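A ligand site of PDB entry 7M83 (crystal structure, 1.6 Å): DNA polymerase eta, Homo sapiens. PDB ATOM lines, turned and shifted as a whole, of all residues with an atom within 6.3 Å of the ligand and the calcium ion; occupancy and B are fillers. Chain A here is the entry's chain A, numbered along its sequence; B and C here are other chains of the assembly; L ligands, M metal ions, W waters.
Residues that only touch the ligand: Asp 18, Ile 51, Ala 52, Ile 117, DT 3 of chain B and DT 5 of chain B.
Within 4 Å of the ligand: Asp 16, Met 17, Asp 18, Cys 19, Phe 20, Phe 21, Ile 51, Ala 52, Tyr 55, Arg 58, Arg 64, Ile 117, Asp 118, Lys 234, DT 3 of chain B, DT 4 of chain B, DT 5 of chain B and DA 8 of chain C.
The nearest printed residue that does not touch the ligand is Glu 119 (4.5 Å).
Lys 234 touches the calcium ion (NZ to CA, 3.95 Å).
Within 4 Å of the calcium ion: Asp 16, Met 17, Asp 118 and Lys 234.
The nearest printed residue that does not touch the calcium ion is Asp 18 (4.5 Å).
OH of Tyr 55 lies within hydrogen-bond range of O2 of the ligand (2.6 Å).
A nitrogen (N3) of the ligand sits at hydrogen-bond distance from O4 of DT 4 of chain B (3.1 Å).
The backbone NH (N) of Cys 19 lies within hydrogen-bond range of an oxygen (O2) of the ligand, 2.8 Å away.
The guanidinium group (NH1) of Arg 58 lies within salt-bridge range of an oxygen (O1) of the ligand (3.1 Å).
NH2 of Arg 64 is in salt-bridge range of O5 of the ligand (3.2 Å).
The backbone NH of Phe 20 is in hydrogen-bond range of an oxygen (O12) of the ligand, 3.4 Å away.
N of Phe 21 lies within hydrogen-bond range of O12 of the ligand.
N6 of DA 8 of chain C sits close to a nitrogen (N3) of the ligand (3.4 Å).
The side-chain amino group (NZ) of Lys 234 lies within salt-bridge range of an oxygen (O2) of the ligand, at 3.4 Å.
Water W6 bridges OD2 of Asp 16 (2.8 Å) and OE2 of Glu 119 (3.3 Å).
Water W1 lies within hydrogen-bond range of O7 of the ligand and NH1 of Arg 64.
Water W8 bridges O7 of the ligand (2.9 Å) and NH1 of Arg 64 (3.4 Å).
Water W5 lies within hydrogen-bond range of N3 of DA 8 of chain C (2.7 Å) and an oxygen (O11) of the ligand (2.9 Å).
The side-chain carboxylate (OD1) of Asp 16 binds the calcium ion (2.2 Å).
The backbone carbonyl oxygen (O) of Met 17 is bound to the calcium ion (2.3 Å).
The calcium ion is bound by OD2 of Asp 118 (2.3 Å).
The calcium ion is bound by an oxygen (O3) of the ligand (2.3 Å).
O4 of the ligand is bound to the calcium ion (2.4 Å).
O8 of the ligand is bound to the calcium ion, at 2.4 Å.
O of Asp 16 is in hydrogen-bond range of NZ of Lys 234 (3.2 Å).
The side-chain amino group (NZ) of Lys 227 lies within salt-bridge range of the side-chain carboxylate (OD2) of Asp 16.
O of Met 17 sits close to NZ of Lys 234 (3.3 Å).
OD1 of Asp 118 lies close to O3' of DA 8 of chain C (2.7 Å).
The side-chain hydroxyl (OH) of Tyr 55 sits at hydrogen-bond distance from the guanidinium group (NH1) of Arg 58 (3.3 Å).
OE1 of Gln 41 sits close to O2 of DT 4 of chain B, 3.1 Å away.
OP1 of DA 8 of chain C lies within salt-bridge range of the side-chain amino group (NZ) of Lys 227.
The side-chain carboxylate (OD1) of Asp 18 is in salt-bridge range of the side-chain amino group (NZ) of Lys 234, 2.9 Å away.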
ATOM      1  N   ASP A  16      10.667   4.391 -10.379  1.00  0.00           N
ATOM      2  CA  ASP A  16       9.982   3.602 -11.404  1.00  0.00           C
ATOM      3  C   ASP A  16      10.880   3.586 -12.635  1.00  0.00           C
ATOM      4  O   ASP A  16      11.093   4.638 -13.259  1.00  0.00           O
ATOM      5  CB  ASP A  16       8.622   4.252 -11.719  1.00  0.00           C
ATOM      6  CG  ASP A  16       7.714   3.405 -12.590  1.00  0.00           C
ATOM      7  OD1 ASP A  16       8.209   2.522 -13.299  1.00  0.00           O
ATOM      8  OD2 ASP A  16       6.485   3.683 -12.602  1.00  0.00           O
ATOM      9  N   MET A  17      11.417   2.414 -13.001  1.00  0.00           N
ATOM     10  CA  MET A  17      12.309   2.358 -14.160  1.00  0.00           C
ATOM     11  C   MET A  17      11.557   2.713 -15.438  1.00  0.00           C
ATOM     12  O   MET A  17      10.406   2.339 -15.606  1.00  0.00           O
ATOM     13  CB  MET A  17      12.955   0.972 -14.295  1.00  0.00           C
ATOM     14  CG  MET A  17      13.611   0.475 -13.010  1.00  0.00           C
ATOM     15  SD  MET A  17      14.911   1.601 -12.388  1.00  0.00           S
ATOM     16  CE  MET A  17      16.034   1.599 -13.722  1.00  0.00           C
ATOM     17  N   ASP A  18      12.217   3.455 -16.336  1.00  0.00           N
ATOM     18  CA  ASP A  18      11.576   3.793 -17.608  1.00  0.00           C
ATOM     19  C   ASP A  18      11.592   2.596 -18.535  1.00  0.00           C
ATOM     20  O   ASP A  18      12.608   1.889 -18.620  1.00  0.00           O
ATOM     21  CB  ASP A  18      12.292   4.971 -18.257  1.00  0.00           C
ATOM     22  CG  ASP A  18      12.235   6.241 -17.396  1.00  0.00           C
ATOM     23  OD1 ASP A  18      11.234   6.450 -16.697  1.00  0.00           O
ATOM     24  OD2 ASP A  18      13.179   7.042 -17.438  1.00  0.00           O
ATOM     25  N   CYS A  19      10.475   2.357 -19.238  1.00  0.00           N
ATOM     26  CA  CYS A  19      10.296   1.267 -20.217  1.00  0.00           C
ATOM     27  C   CYS A  19      11.245   0.097 -19.912  1.00  0.00           C
ATOM     28  O   CYS A  19      12.131  -0.231 -20.694  1.00  0.00           O
ATOM     29  CB  CYS A  19      10.467   1.776 -21.660  1.00  0.00           C
ATOM     30  SG  CYS A  19      11.952   2.670 -22.087  1.00  0.00           S
ATOM     31  N   PHE A  20      11.048  -0.535 -18.752  1.00  0.00           N
ATOM     32  CA  PHE A  20      12.113  -1.318 -18.143  1.00  0.00           C
ATOM     33  C   PHE A  20      12.629  -2.469 -19.009  1.00  0.00           C
ATOM     34  O   PHE A  20      13.842  -2.574 -19.225  1.00  0.00           O
ATOM     35  CB  PHE A  20      11.647  -1.855 -16.789  1.00  0.00           C
ATOM     36  CG  PHE A  20      12.729  -2.603 -16.049  1.00  0.00           C
ATOM     37  CD1 PHE A  20      13.991  -2.038 -15.871  1.00  0.00           C
ATOM     38  CD2 PHE A  20      12.487  -3.877 -15.556  1.00  0.00           C
ATOM     39  CE1 PHE A  20      14.988  -2.722 -15.176  1.00  0.00           C
ATOM     40  CE2 PHE A  20      13.500  -4.572 -14.851  1.00  0.00           C
ATOM     41  CZ  PHE A  20      14.743  -3.970 -14.669  1.00  0.00           C
ATOM     42  N   PHE A  21      11.737  -3.347 -19.481  1.00  0.00           N
ATOM     43  CA  PHE A  21      12.263  -4.492 -20.238  1.00  0.00           C
ATOM     44  C   PHE A  21      12.962  -4.029 -21.519  1.00  0.00           C
ATOM     45  O   PHE A  21      13.908  -4.668 -21.992  1.00  0.00           O
ATOM     46  CB  PHE A  21      11.164  -5.494 -20.609  1.00  0.00           C
ATOM     47  CG  PHE A  21      10.591  -6.290 -19.451  1.00  0.00           C
ATOM     48  CD1 PHE A  21      10.781  -5.922 -18.128  1.00  0.00           C
ATOM     49  CD2 PHE A  21       9.818  -7.411 -19.711  1.00  0.00           C
ATOM     50  CE1 PHE A  21      10.207  -6.667 -17.092  1.00  0.00           C
ATOM     51  CE2 PHE A  21       9.243  -8.168 -18.668  1.00  0.00           C
ATOM     52  CZ  PHE A  21       9.453  -7.788 -17.363  1.00  0.00           C
ATOM     53  N   VAL A  22      12.471  -2.940 -22.114  1.00  0.00           N
ATOM     54  CA  VAL A  22      13.132  -2.365 -23.282  1.00  0.00           C
ATOM     55  C   VAL A  22      14.548  -1.941 -22.923  1.00  0.00           C
ATOM     56  O   VAL A  22      15.506  -2.228 -23.650  1.00  0.00           O
ATOM     57  CB  VAL A  22      12.323  -1.191 -23.836  1.00  0.00           C
ATOM     58  CG1 VAL A  22      13.153  -0.316 -24.798  1.00  0.00           C
ATOM     59  CG2 VAL A  22      11.045  -1.677 -24.499  1.00  0.00           C
ATOM     60  N   GLN A  41       6.454 -11.189 -26.404  1.00  0.00           N
ATOM     61  CA  GLN A  41       6.438 -12.582 -25.932  1.00  0.00           C
ATOM     62  C   GLN A  41       5.766 -13.385 -27.034  1.00  0.00           C
ATOM     63  O   GLN A  41       4.661 -13.003 -27.435  1.00  0.00           O
ATOM     64  CB  GLN A  41       5.627 -12.783 -24.646  1.00  0.00           C
ATOM     65  CG  GLN A  41       6.204 -12.125 -23.416  1.00  0.00           C
ATOM     66  CD  GLN A  41       5.389 -12.473 -22.200  1.00  0.00           C
ATOM     67  OE1 GLN A  41       4.169 -12.387 -22.201  1.00  0.00           O
ATOM     68  NE2 GLN A  41       6.082 -12.872 -21.148  1.00  0.00           N
ATOM     69  N   ILE A  51       4.842  -6.390 -24.557  1.00  0.00           N
ATOM     70  CA  ILE A  51       4.774  -6.137 -23.114  1.00  0.00           C
ATOM     71  C   ILE A  51       5.551  -4.903 -22.675  1.00  0.00           C
ATOM     72  O   ILE A  51       5.381  -4.469 -21.534  1.00  0.00           O
ATOM     73  CB  ILE A  51       5.189  -7.382 -22.293  1.00  0.00           C
ATOM     74  CG1 ILE A  51       6.626  -7.833 -22.593  1.00  0.00           C
ATOM     75  CG2 ILE A  51       4.177  -8.513 -22.503  1.00  0.00           C
ATOM     76  CD1 ILE A  51       7.119  -8.896 -21.588  1.00  0.00           C
ATOM     77  N   ALA A  52       6.383  -4.300 -23.525  1.00  0.00           N
ATOM     78  CA  ALA A  52       7.090  -3.071 -23.149  1.00  0.00           C
ATOM     79  C   ALA A  52       7.437  -2.312 -24.427  1.00  0.00           C
ATOM     80  O   ALA A  52       7.689  -2.937 -25.472  1.00  0.00           O
ATOM     81  CB  ALA A  52       8.365  -3.351 -22.331  1.00  0.00           C
ATOM     82  N   VAL A  53       7.455  -0.971 -24.330  1.00  0.00           N
ATOM     83  CA  VAL A  53       7.555  -0.099 -25.504  1.00  0.00           C
ATOM     84  C   VAL A  53       8.456   1.091 -25.229  1.00  0.00           C
ATOM     85  O   VAL A  53       8.251   1.813 -24.249  1.00  0.00           O
ATOM     86  CB  VAL A  53       6.166   0.424 -25.916  1.00  0.00           C
ATOM     87  CG1 VAL A  53       6.244   1.193 -27.229  1.00  0.00           C
ATOM     88  CG2 VAL A  53       5.163  -0.710 -26.045  1.00  0.00           C
ATOM     89  N   TYR A  55      10.049   4.867 -25.636  1.00  0.00           N
ATOM     90  CA  TYR A  55       9.348   6.144 -25.812  1.00  0.00           C
ATOM     91  C   TYR A  55       9.324   6.584 -27.283  1.00  0.00           C
ATOM     92  O   TYR A  55       8.328   7.156 -27.760  1.00  0.00           O
ATOM     93  CB  TYR A  55       9.957   7.218 -24.877  1.00  0.00           C
ATOM     94  CG  TYR A  55       9.468   7.021 -23.454  1.00  0.00           C
ATOM     95  CD1 TYR A  55       9.995   6.028 -22.631  1.00  0.00           C
ATOM     96  CD2 TYR A  55       8.360   7.738 -22.991  1.00  0.00           C
ATOM     97  CE1 TYR A  55       9.473   5.809 -21.350  1.00  0.00           C
ATOM     98  CE2 TYR A  55       7.859   7.530 -21.727  1.00  0.00           C
ATOM     99  CZ  TYR A  55       8.404   6.574 -20.909  1.00  0.00           C
ATOM    100  OH  TYR A  55       7.893   6.363 -19.654  1.00  0.00           O
ATOM    101  N   ARG A  58       6.418   4.753 -28.610  1.00  0.00           N
ATOM    102  CA  ARG A  58       5.152   5.296 -28.123  1.00  0.00           C
ATOM    103  C   ARG A  58       4.722   6.504 -28.953  1.00  0.00           C
ATOM    104  O   ARG A  58       3.518   6.756 -29.104  1.00  0.00           O
ATOM    105  CB  ARG A  58       5.239   5.696 -26.654  1.00  0.00           C
ATOM    106  CG  ARG A  58       5.568   4.551 -25.750  1.00  0.00           C
ATOM    107  CD  ARG A  58       5.702   4.991 -24.288  1.00  0.00           C
ATOM    108  NE  ARG A  58       6.381   3.935 -23.530  1.00  0.00           N
ATOM    109  CZ  ARG A  58       6.381   3.810 -22.212  1.00  0.00           C
ATOM    110  NH1 ARG A  58       5.717   4.684 -21.441  1.00  0.00           N
ATOM    111  NH2 ARG A  58       7.062   2.801 -21.656  1.00  0.00           N
ATOM    112  N   ARG A  64       1.387  -1.334 -25.019  1.00  0.00           N
ATOM    113  CA  ARG A  64       1.359  -2.702 -24.478  1.00  0.00           C
ATOM    114  C   ARG A  64       0.018  -3.338 -24.835  1.00  0.00           C
ATOM    115  O   ARG A  64      -0.911  -2.584 -25.059  1.00  0.00           O
ATOM    116  CB  ARG A  64       1.491  -2.624 -22.946  1.00  0.00           C
ATOM    117  CG  ARG A  64       1.515  -3.920 -22.174  1.00  0.00           C
ATOM    118  CD  ARG A  64       1.672  -3.594 -20.706  1.00  0.00           C
ATOM    119  NE  ARG A  64       3.042  -3.169 -20.520  1.00  0.00           N
ATOM    120  CZ  ARG A  64       3.432  -2.077 -19.891  1.00  0.00           C
ATOM    121  NH1 ARG A  64       2.548  -1.258 -19.339  1.00  0.00           N
ATOM    122  NH2 ARG A  64       4.715  -1.811 -19.813  1.00  0.00           N
ATOM    123  N   ILE A 117       8.419  -5.403 -10.271  1.00  0.00           N
ATOM    124  CA  ILE A 117       9.720  -5.779 -10.819  1.00  0.00           C
ATOM    125  C   ILE A 117      10.636  -4.580 -11.045  1.00  0.00           C
ATOM    126  O   ILE A 117      11.857  -4.693 -10.921  1.00  0.00           O
ATOM    127  CB  ILE A 117       9.552  -6.568 -12.138  1.00  0.00           C
ATOM    128  CG1 ILE A 117      10.849  -7.312 -12.445  1.00  0.00           C
ATOM    129  CG2 ILE A 117       9.133  -5.675 -13.292  1.00  0.00           C
ATOM    130  CD1 ILE A 117      10.689  -8.477 -13.433  1.00  0.00           C
ATOM    131  N   ASP A 118      10.065  -3.403 -11.267  1.00  0.00           N
ATOM    132  CA  ASP A 118      10.878  -2.233 -11.576  1.00  0.00           C
ATOM    133  C   ASP A 118      10.480  -1.011 -10.775  1.00  0.00           C
ATOM    134  O   ASP A 118      10.787   0.121 -11.175  1.00  0.00           O
ATOM    135  CB  ASP A 118      10.783  -1.984 -13.077  1.00  0.00           C
ATOM    136  CG  ASP A 118       9.525  -1.229 -13.433  1.00  0.00           C
ATOM    137  OD1 ASP A 118       8.480  -1.502 -12.764  1.00  0.00           O
ATOM    138  OD2 ASP A 118       9.549  -0.368 -14.348  1.00  0.00           O
ATOM    139  N   GLU A 119       9.802  -1.214  -9.638  1.00  0.00           N
ATOM    140  CA  GLU A 119       9.360  -0.085  -8.823  1.00  0.00           C
ATOM    141  C   GLU A 119       9.695  -0.374  -7.384  1.00  0.00           C
ATOM    142  O   GLU A 119       9.448  -1.484  -6.895  1.00  0.00           O
ATOM    143  CB  GLU A 119       7.867   0.137  -8.868  1.00  0.00           C
ATOM    144  CG  GLU A 119       7.319   0.691 -10.133  1.00  0.00           C
ATOM    145  CD  GLU A 119       5.858   1.075  -9.967  1.00  0.00           C
ATOM    146  OE1 GLU A 119       5.446   1.209  -8.793  1.00  0.00           O
ATOM    147  OE2 GLU A 119       5.138   1.242 -10.970  1.00  0.00           O
ATOM    148  N   LYS A 227       3.894   8.023  -5.802  1.00  0.00           N
ATOM    149  CA  LYS A 227       3.595   7.278  -7.016  1.00  0.00           C
ATOM    150  C   LYS A 227       2.942   8.187  -8.048  1.00  0.00           C
ATOM    151  O   LYS A 227       3.316   8.167  -9.230  1.00  0.00           O
ATOM    152  CB  LYS A 227       2.706   6.084  -6.678  1.00  0.00           C
ATOM    153  CG  LYS A 227       2.151   5.308  -7.867  1.00  0.00           C
ATOM    154  CD  LYS A 227       3.247   4.664  -8.686  1.00  0.00           C
ATOM    155  CE  LYS A 227       2.677   3.694  -9.702  1.00  0.00           C
ATOM    156  NZ  LYS A 227       3.702   3.395 -10.733  1.00  0.00           N
ATOM    157  N   LYS A 234       7.618  11.678 -16.365  1.00  0.00           N
ATOM    158  CA  LYS A 234       8.395  10.559 -16.860  1.00  0.00           C
ATOM    159  C   LYS A 234       8.480  10.733 -18.386  1.00  0.00           C
ATOM    160  O   LYS A 234       7.555  11.270 -18.994  1.00  0.00           O
ATOM    161  CB  LYS A 234       7.687   9.281 -16.351  1.00  0.00           C
ATOM    162  CG  LYS A 234       8.267   7.914 -16.577  1.00  0.00           C
ATOM    163  CD  LYS A 234       7.226   6.839 -16.656  1.00  0.00           C
ATOM    164  CE  LYS A 234       7.491   5.890 -15.458  1.00  0.00           C
ATOM    165  NZ  LYS A 234       8.913   5.296 -15.485  1.00  0.00           N
ATOM    166  N   PRO A 235       9.579  10.279 -19.048  1.00  0.00           N
ATOM    167  CA  PRO A 235      10.710   9.594 -18.415  1.00  0.00           C
ATOM    168  C   PRO A 235      11.920  10.444 -18.043  1.00  0.00           C
ATOM    169  O   PRO A 235      12.074  11.609 -18.442  1.00  0.00           O
ATOM    170  CB  PRO A 235      11.165   8.648 -19.518  1.00  0.00           C
ATOM    171  CG  PRO A 235      10.978   9.514 -20.788  1.00  0.00           C
ATOM    172  CD  PRO A 235       9.746  10.339 -20.514  1.00  0.00           C
ATOM    173  P    DT B   3      -7.503 -11.341 -27.238  1.00  0.00           P
ATOM    174  OP1  DT B   3      -8.924 -11.700 -27.053  1.00  0.00           O
ATOM    175  OP2  DT B   3      -7.121 -10.180 -28.049  1.00  0.00           O
ATOM    176  O5'  DT B   3      -6.888 -11.178 -25.777  1.00  0.00           O
ATOM    177  C5'  DT B   3      -5.771 -10.318 -25.573  1.00  0.00           C
ATOM    178  C4'  DT B   3      -4.499 -11.116 -25.681  1.00  0.00           C
ATOM    179  O4'  DT B   3      -3.380 -10.216 -25.520  1.00  0.00           O
ATOM    180  C3'  DT B   3      -4.348 -12.172 -24.574  1.00  0.00           C
ATOM    181  O3'  DT B   3      -3.753 -13.403 -25.000  1.00  0.00           O
ATOM    182  C2'  DT B   3      -3.451 -11.466 -23.580  1.00  0.00           C
ATOM    183  C1'  DT B   3      -2.538 -10.726 -24.518  1.00  0.00           C
ATOM    184  N1   DT B   3      -1.841  -9.607 -23.869  1.00  0.00           N
ATOM    185  C2   DT B   3      -0.500  -9.494 -24.109  1.00  0.00           C
ATOM    186  O2   DT B   3       0.106 -10.228 -24.878  1.00  0.00           O
ATOM    187  N3   DT B   3       0.113  -8.452 -23.452  1.00  0.00           N
ATOM    188  C4   DT B   3      -0.470  -7.562 -22.580  1.00  0.00           C
ATOM    189  O4   DT B   3       0.198  -6.677 -22.070  1.00  0.00           O
ATOM    190  C5   DT B   3      -1.893  -7.737 -22.376  1.00  0.00           C
ATOM    191  C7   DT B   3      -2.624  -6.808 -21.467  1.00  0.00           C
ATOM    192  C6   DT B   3      -2.496  -8.750 -23.024  1.00  0.00           C
ATOM    193  P    DT B   4      -3.365 -14.595 -23.941  1.00  0.00           P
ATOM    194  OP1  DT B   4      -3.235 -15.856 -24.688  1.00  0.00           O
ATOM    195  OP2  DT B   4      -4.260 -14.478 -22.761  1.00  0.00           O
ATOM    196  O5'  DT B   4      -1.952 -14.156 -23.374  1.00  0.00           O
ATOM    197  C5'  DT B   4      -0.811 -14.269 -24.164  1.00  0.00           C
ATOM    198  C4'  DT B   4       0.373 -14.347 -23.257  1.00  0.00           C
ATOM    199  O4'  DT B   4       0.515 -13.041 -22.647  1.00  0.00           O
ATOM    200  C3'  DT B   4       0.256 -15.330 -22.092  1.00  0.00           C
ATOM    201  O3'  DT B   4       1.529 -15.937 -21.944  1.00  0.00           O
ATOM    202  C2'  DT B   4      -0.125 -14.445 -20.909  1.00  0.00           C
ATOM    203  C1'  DT B   4       0.630 -13.181 -21.251  1.00  0.00           C
ATOM    204  N1   DT B   4       0.059 -11.940 -20.634  1.00  0.00           N
ATOM    205  C2   DT B   4       0.924 -10.976 -20.204  1.00  0.00           C
ATOM    206  O2   DT B   4       2.116 -11.128 -20.207  1.00  0.00           O
ATOM    207  N3   DT B   4       0.332  -9.854 -19.696  1.00  0.00           N
ATOM    208  C4   DT B   4      -1.012  -9.578 -19.622  1.00  0.00           C
ATOM    209  O4   DT B   4      -1.433  -8.523 -19.154  1.00  0.00           O
ATOM    210  C5   DT B   4      -1.884 -10.612 -20.145  1.00  0.00           C
ATOM    211  C7   DT B   4      -3.381 -10.421 -20.105  1.00  0.00           C
ATOM    212  C6   DT B   4      -1.308 -11.726 -20.627  1.00  0.00           C
ATOM    213  P    DT B   5       1.819 -17.042 -20.825  1.00  0.00           P
ATOM    214  OP1  DT B   5       2.802 -17.964 -21.408  1.00  0.00           O
ATOM    215  OP2  DT B   5       0.527 -17.520 -20.283  1.00  0.00           O
ATOM    216  O5'  DT B   5       2.573 -16.203 -19.687  1.00  0.00           O
ATOM    217  C5'  DT B   5       3.878 -15.718 -19.946  1.00  0.00           C
ATOM    218  C4'  DT B   5       4.400 -14.982 -18.733  1.00  0.00           C
ATOM    219  O4'  DT B   5       3.603 -13.793 -18.516  1.00  0.00           O
ATOM    220  C3'  DT B   5       4.323 -15.788 -17.427  1.00  0.00           C
ATOM    221  O3'  DT B   5       5.501 -15.515 -16.641  1.00  0.00           O
ATOM    222  C2'  DT B   5       3.071 -15.214 -16.758  1.00  0.00           C
ATOM    223  C1'  DT B   5       3.227 -13.755 -17.161  1.00  0.00           C
ATOM    224  N1   DT B   5       2.017 -12.944 -17.006  1.00  0.00           N
ATOM    225  C2   DT B   5       2.178 -11.637 -16.630  1.00  0.00           C
ATOM    226  O2   DT B   5       3.281 -11.136 -16.423  1.00  0.00           O
ATOM    227  N3   DT B   5       1.030 -10.929 -16.498  1.00  0.00           N
ATOM    228  C4   DT B   5      -0.258 -11.384 -16.718  1.00  0.00           C
ATOM    229  O4   DT B   5      -1.236 -10.661 -16.584  1.00  0.00           O
ATOM    230  C5   DT B   5      -0.364 -12.774 -17.140  1.00  0.00           C
ATOM    231  C7   DT B   5      -1.715 -13.388 -17.405  1.00  0.00           C
ATOM    232  C6   DT B   5       0.781 -13.482 -17.259  1.00  0.00           C
ATOM    233  P    DA C   8       1.458  -0.034 -10.643  1.00  0.00           P
ATOM    234  OP1  DA C   8       2.549   0.477  -9.791  1.00  0.00           O
ATOM    235  OP2  DA C   8       0.774   0.864 -11.600  1.00  0.00           O
ATOM    236  O5'  DA C   8       1.994  -1.290 -11.460  1.00  0.00           O
ATOM    237  C5'  DA C   8       3.070  -1.151 -12.338  1.00  0.00           C
ATOM    238  C4'  DA C   8       4.020  -2.290 -12.104  1.00  0.00           C
ATOM    239  O4'  DA C   8       3.255  -3.532 -11.994  1.00  0.00           O
ATOM    240  C3'  DA C   8       5.065  -2.525 -13.175  1.00  0.00           C
ATOM    241  O3'  DA C   8       6.241  -3.072 -12.622  1.00  0.00           O
ATOM    242  C2'  DA C   8       4.359  -3.521 -14.094  1.00  0.00           C
ATOM    243  C1'  DA C   8       3.586  -4.379 -13.093  1.00  0.00           C
ATOM    244  N9   DA C   8       2.354  -4.949 -13.624  1.00  0.00           N
ATOM    245  C8   DA C   8       1.100  -4.401 -13.588  1.00  0.00           C
ATOM    246  N7   DA C   8       0.184  -5.141 -14.153  1.00  0.00           N
ATOM    247  C5   DA C   8       0.884  -6.275 -14.576  1.00  0.00           C
ATOM    248  C6   DA C   8       0.469  -7.445 -15.230  1.00  0.00           C
ATOM    249  N6   DA C   8      -0.789  -7.698 -15.578  1.00  0.00           N
ATOM    250  N1   DA C   8       1.413  -8.362 -15.504  1.00  0.00           N
ATOM    251  C2   DA C   8       2.682  -8.117 -15.155  1.00  0.00           C
ATOM    252  N3   DA C   8       3.183  -7.054 -14.527  1.00  0.00           N
ATOM    253  C4   DA C   8       2.218  -6.158 -14.263  1.00  0.00           C
HETATM  254  P1  LIG L   1       7.129   3.201 -18.113  1.00  0.00           P
HETATM  255  O1  LIG L   1       5.840   3.879 -18.466  1.00  0.00           O
HETATM  256  O2  LIG L   1       8.278   4.024 -18.542  1.00  0.00           O
HETATM  257  O3  LIG L   1       7.243   2.882 -16.657  1.00  0.00           O
HETATM  258  P2  LIG L   1       7.358   0.350 -18.351  1.00  0.00           P
HETATM  259  O4  LIG L   1       8.470   0.263 -17.335  1.00  0.00           O
HETATM  260  O5  LIG L   1       7.617  -0.537 -19.505  1.00  0.00           O
HETATM  261  O6  LIG L   1       7.184   1.835 -18.873  1.00  0.00           O
HETATM  262  P3  LIG L   1       5.649  -0.629 -16.304  1.00  0.00           P
HETATM  263  O7  LIG L   1       4.164  -0.617 -16.172  1.00  0.00           O
HETATM  264  O8  LIG L   1       6.303   0.165 -15.234  1.00  0.00           O
HETATM  265  O9  LIG L   1       5.987  -0.059 -17.696  1.00  0.00           O
HETATM  266  O10 LIG L   1       6.143  -2.123 -16.285  1.00  0.00           O
HETATM  267  C1  LIG L   1       7.436  -2.491 -15.979  1.00  0.00           C
HETATM  268  C2  LIG L   1       7.791  -3.750 -16.736  1.00  0.00           C
HETATM  269  O11 LIG L   1       6.861  -4.795 -16.364  1.00  0.00           O
HETATM  270  C3  LIG L   1       7.540  -3.516 -18.223  1.00  0.00           C
HETATM  271  O12 LIG L   1       8.731  -3.080 -18.854  1.00  0.00           O
HETATM  272  C4  LIG L   1       7.202  -4.920 -18.687  1.00  0.00           C
HETATM  273  C5  LIG L   1       6.493  -5.507 -17.549  1.00  0.00           C
HETATM  274  N1  LIG L   1       5.020  -5.425 -17.675  1.00  0.00           N
HETATM  275  C6  LIG L   1       4.255  -4.363 -17.413  1.00  0.00           C
HETATM  276  N2  LIG L   1       2.974  -4.638 -17.635  1.00  0.00           N
HETATM  277  C7  LIG L   1       2.907  -5.934 -18.044  1.00  0.00           C
HETATM  278  C8  LIG L   1       1.875  -6.773 -18.421  1.00  0.00           C
HETATM  279  N3  LIG L   1       0.619  -6.331 -18.411  1.00  0.00           N
HETATM  280  N4  LIG L   1       2.162  -7.993 -18.774  1.00  0.00           N
HETATM  281  C9  LIG L   1       3.428  -8.406 -18.774  1.00  0.00           C
HETATM  282  N5  LIG L   1       4.450  -7.690 -18.441  1.00  0.00           N
HETATM  283  C10 LIG L   1       4.213  -6.434 -18.072  1.00  0.00           C
HETATM  284 CA    CA M   1       8.363   1.391 -15.237  1.00  0.00          CA
HETATM  285  O   HOH W   1       2.508   1.295 -17.538  1.00  0.00           O
HETATM  286  O   HOH W   2       4.276   4.217 -16.154  1.00  0.00           O
HETATM  287  O   HOH W   3      -0.920  -3.807 -17.983  1.00  0.00           O
HETATM  288  O   HOH W   4       6.447  -0.121 -21.867  1.00  0.00           O
HETATM  289  O   HOH W   5       5.904  -6.753 -14.381  1.00  0.00           O
HETATM  290  O   HOH W   6       4.711   2.184 -14.146  1.00  0.00           O
HETATM  291  O   HOH W   7       3.591   2.563 -19.423  1.00  0.00           O
HETATM  292  O   HOH W   8       1.832  -2.336 -16.204  1.00  0.00           O
HETATM  293  O   HOH W   9       6.446  -9.541 -17.553  1.00  0.00           O
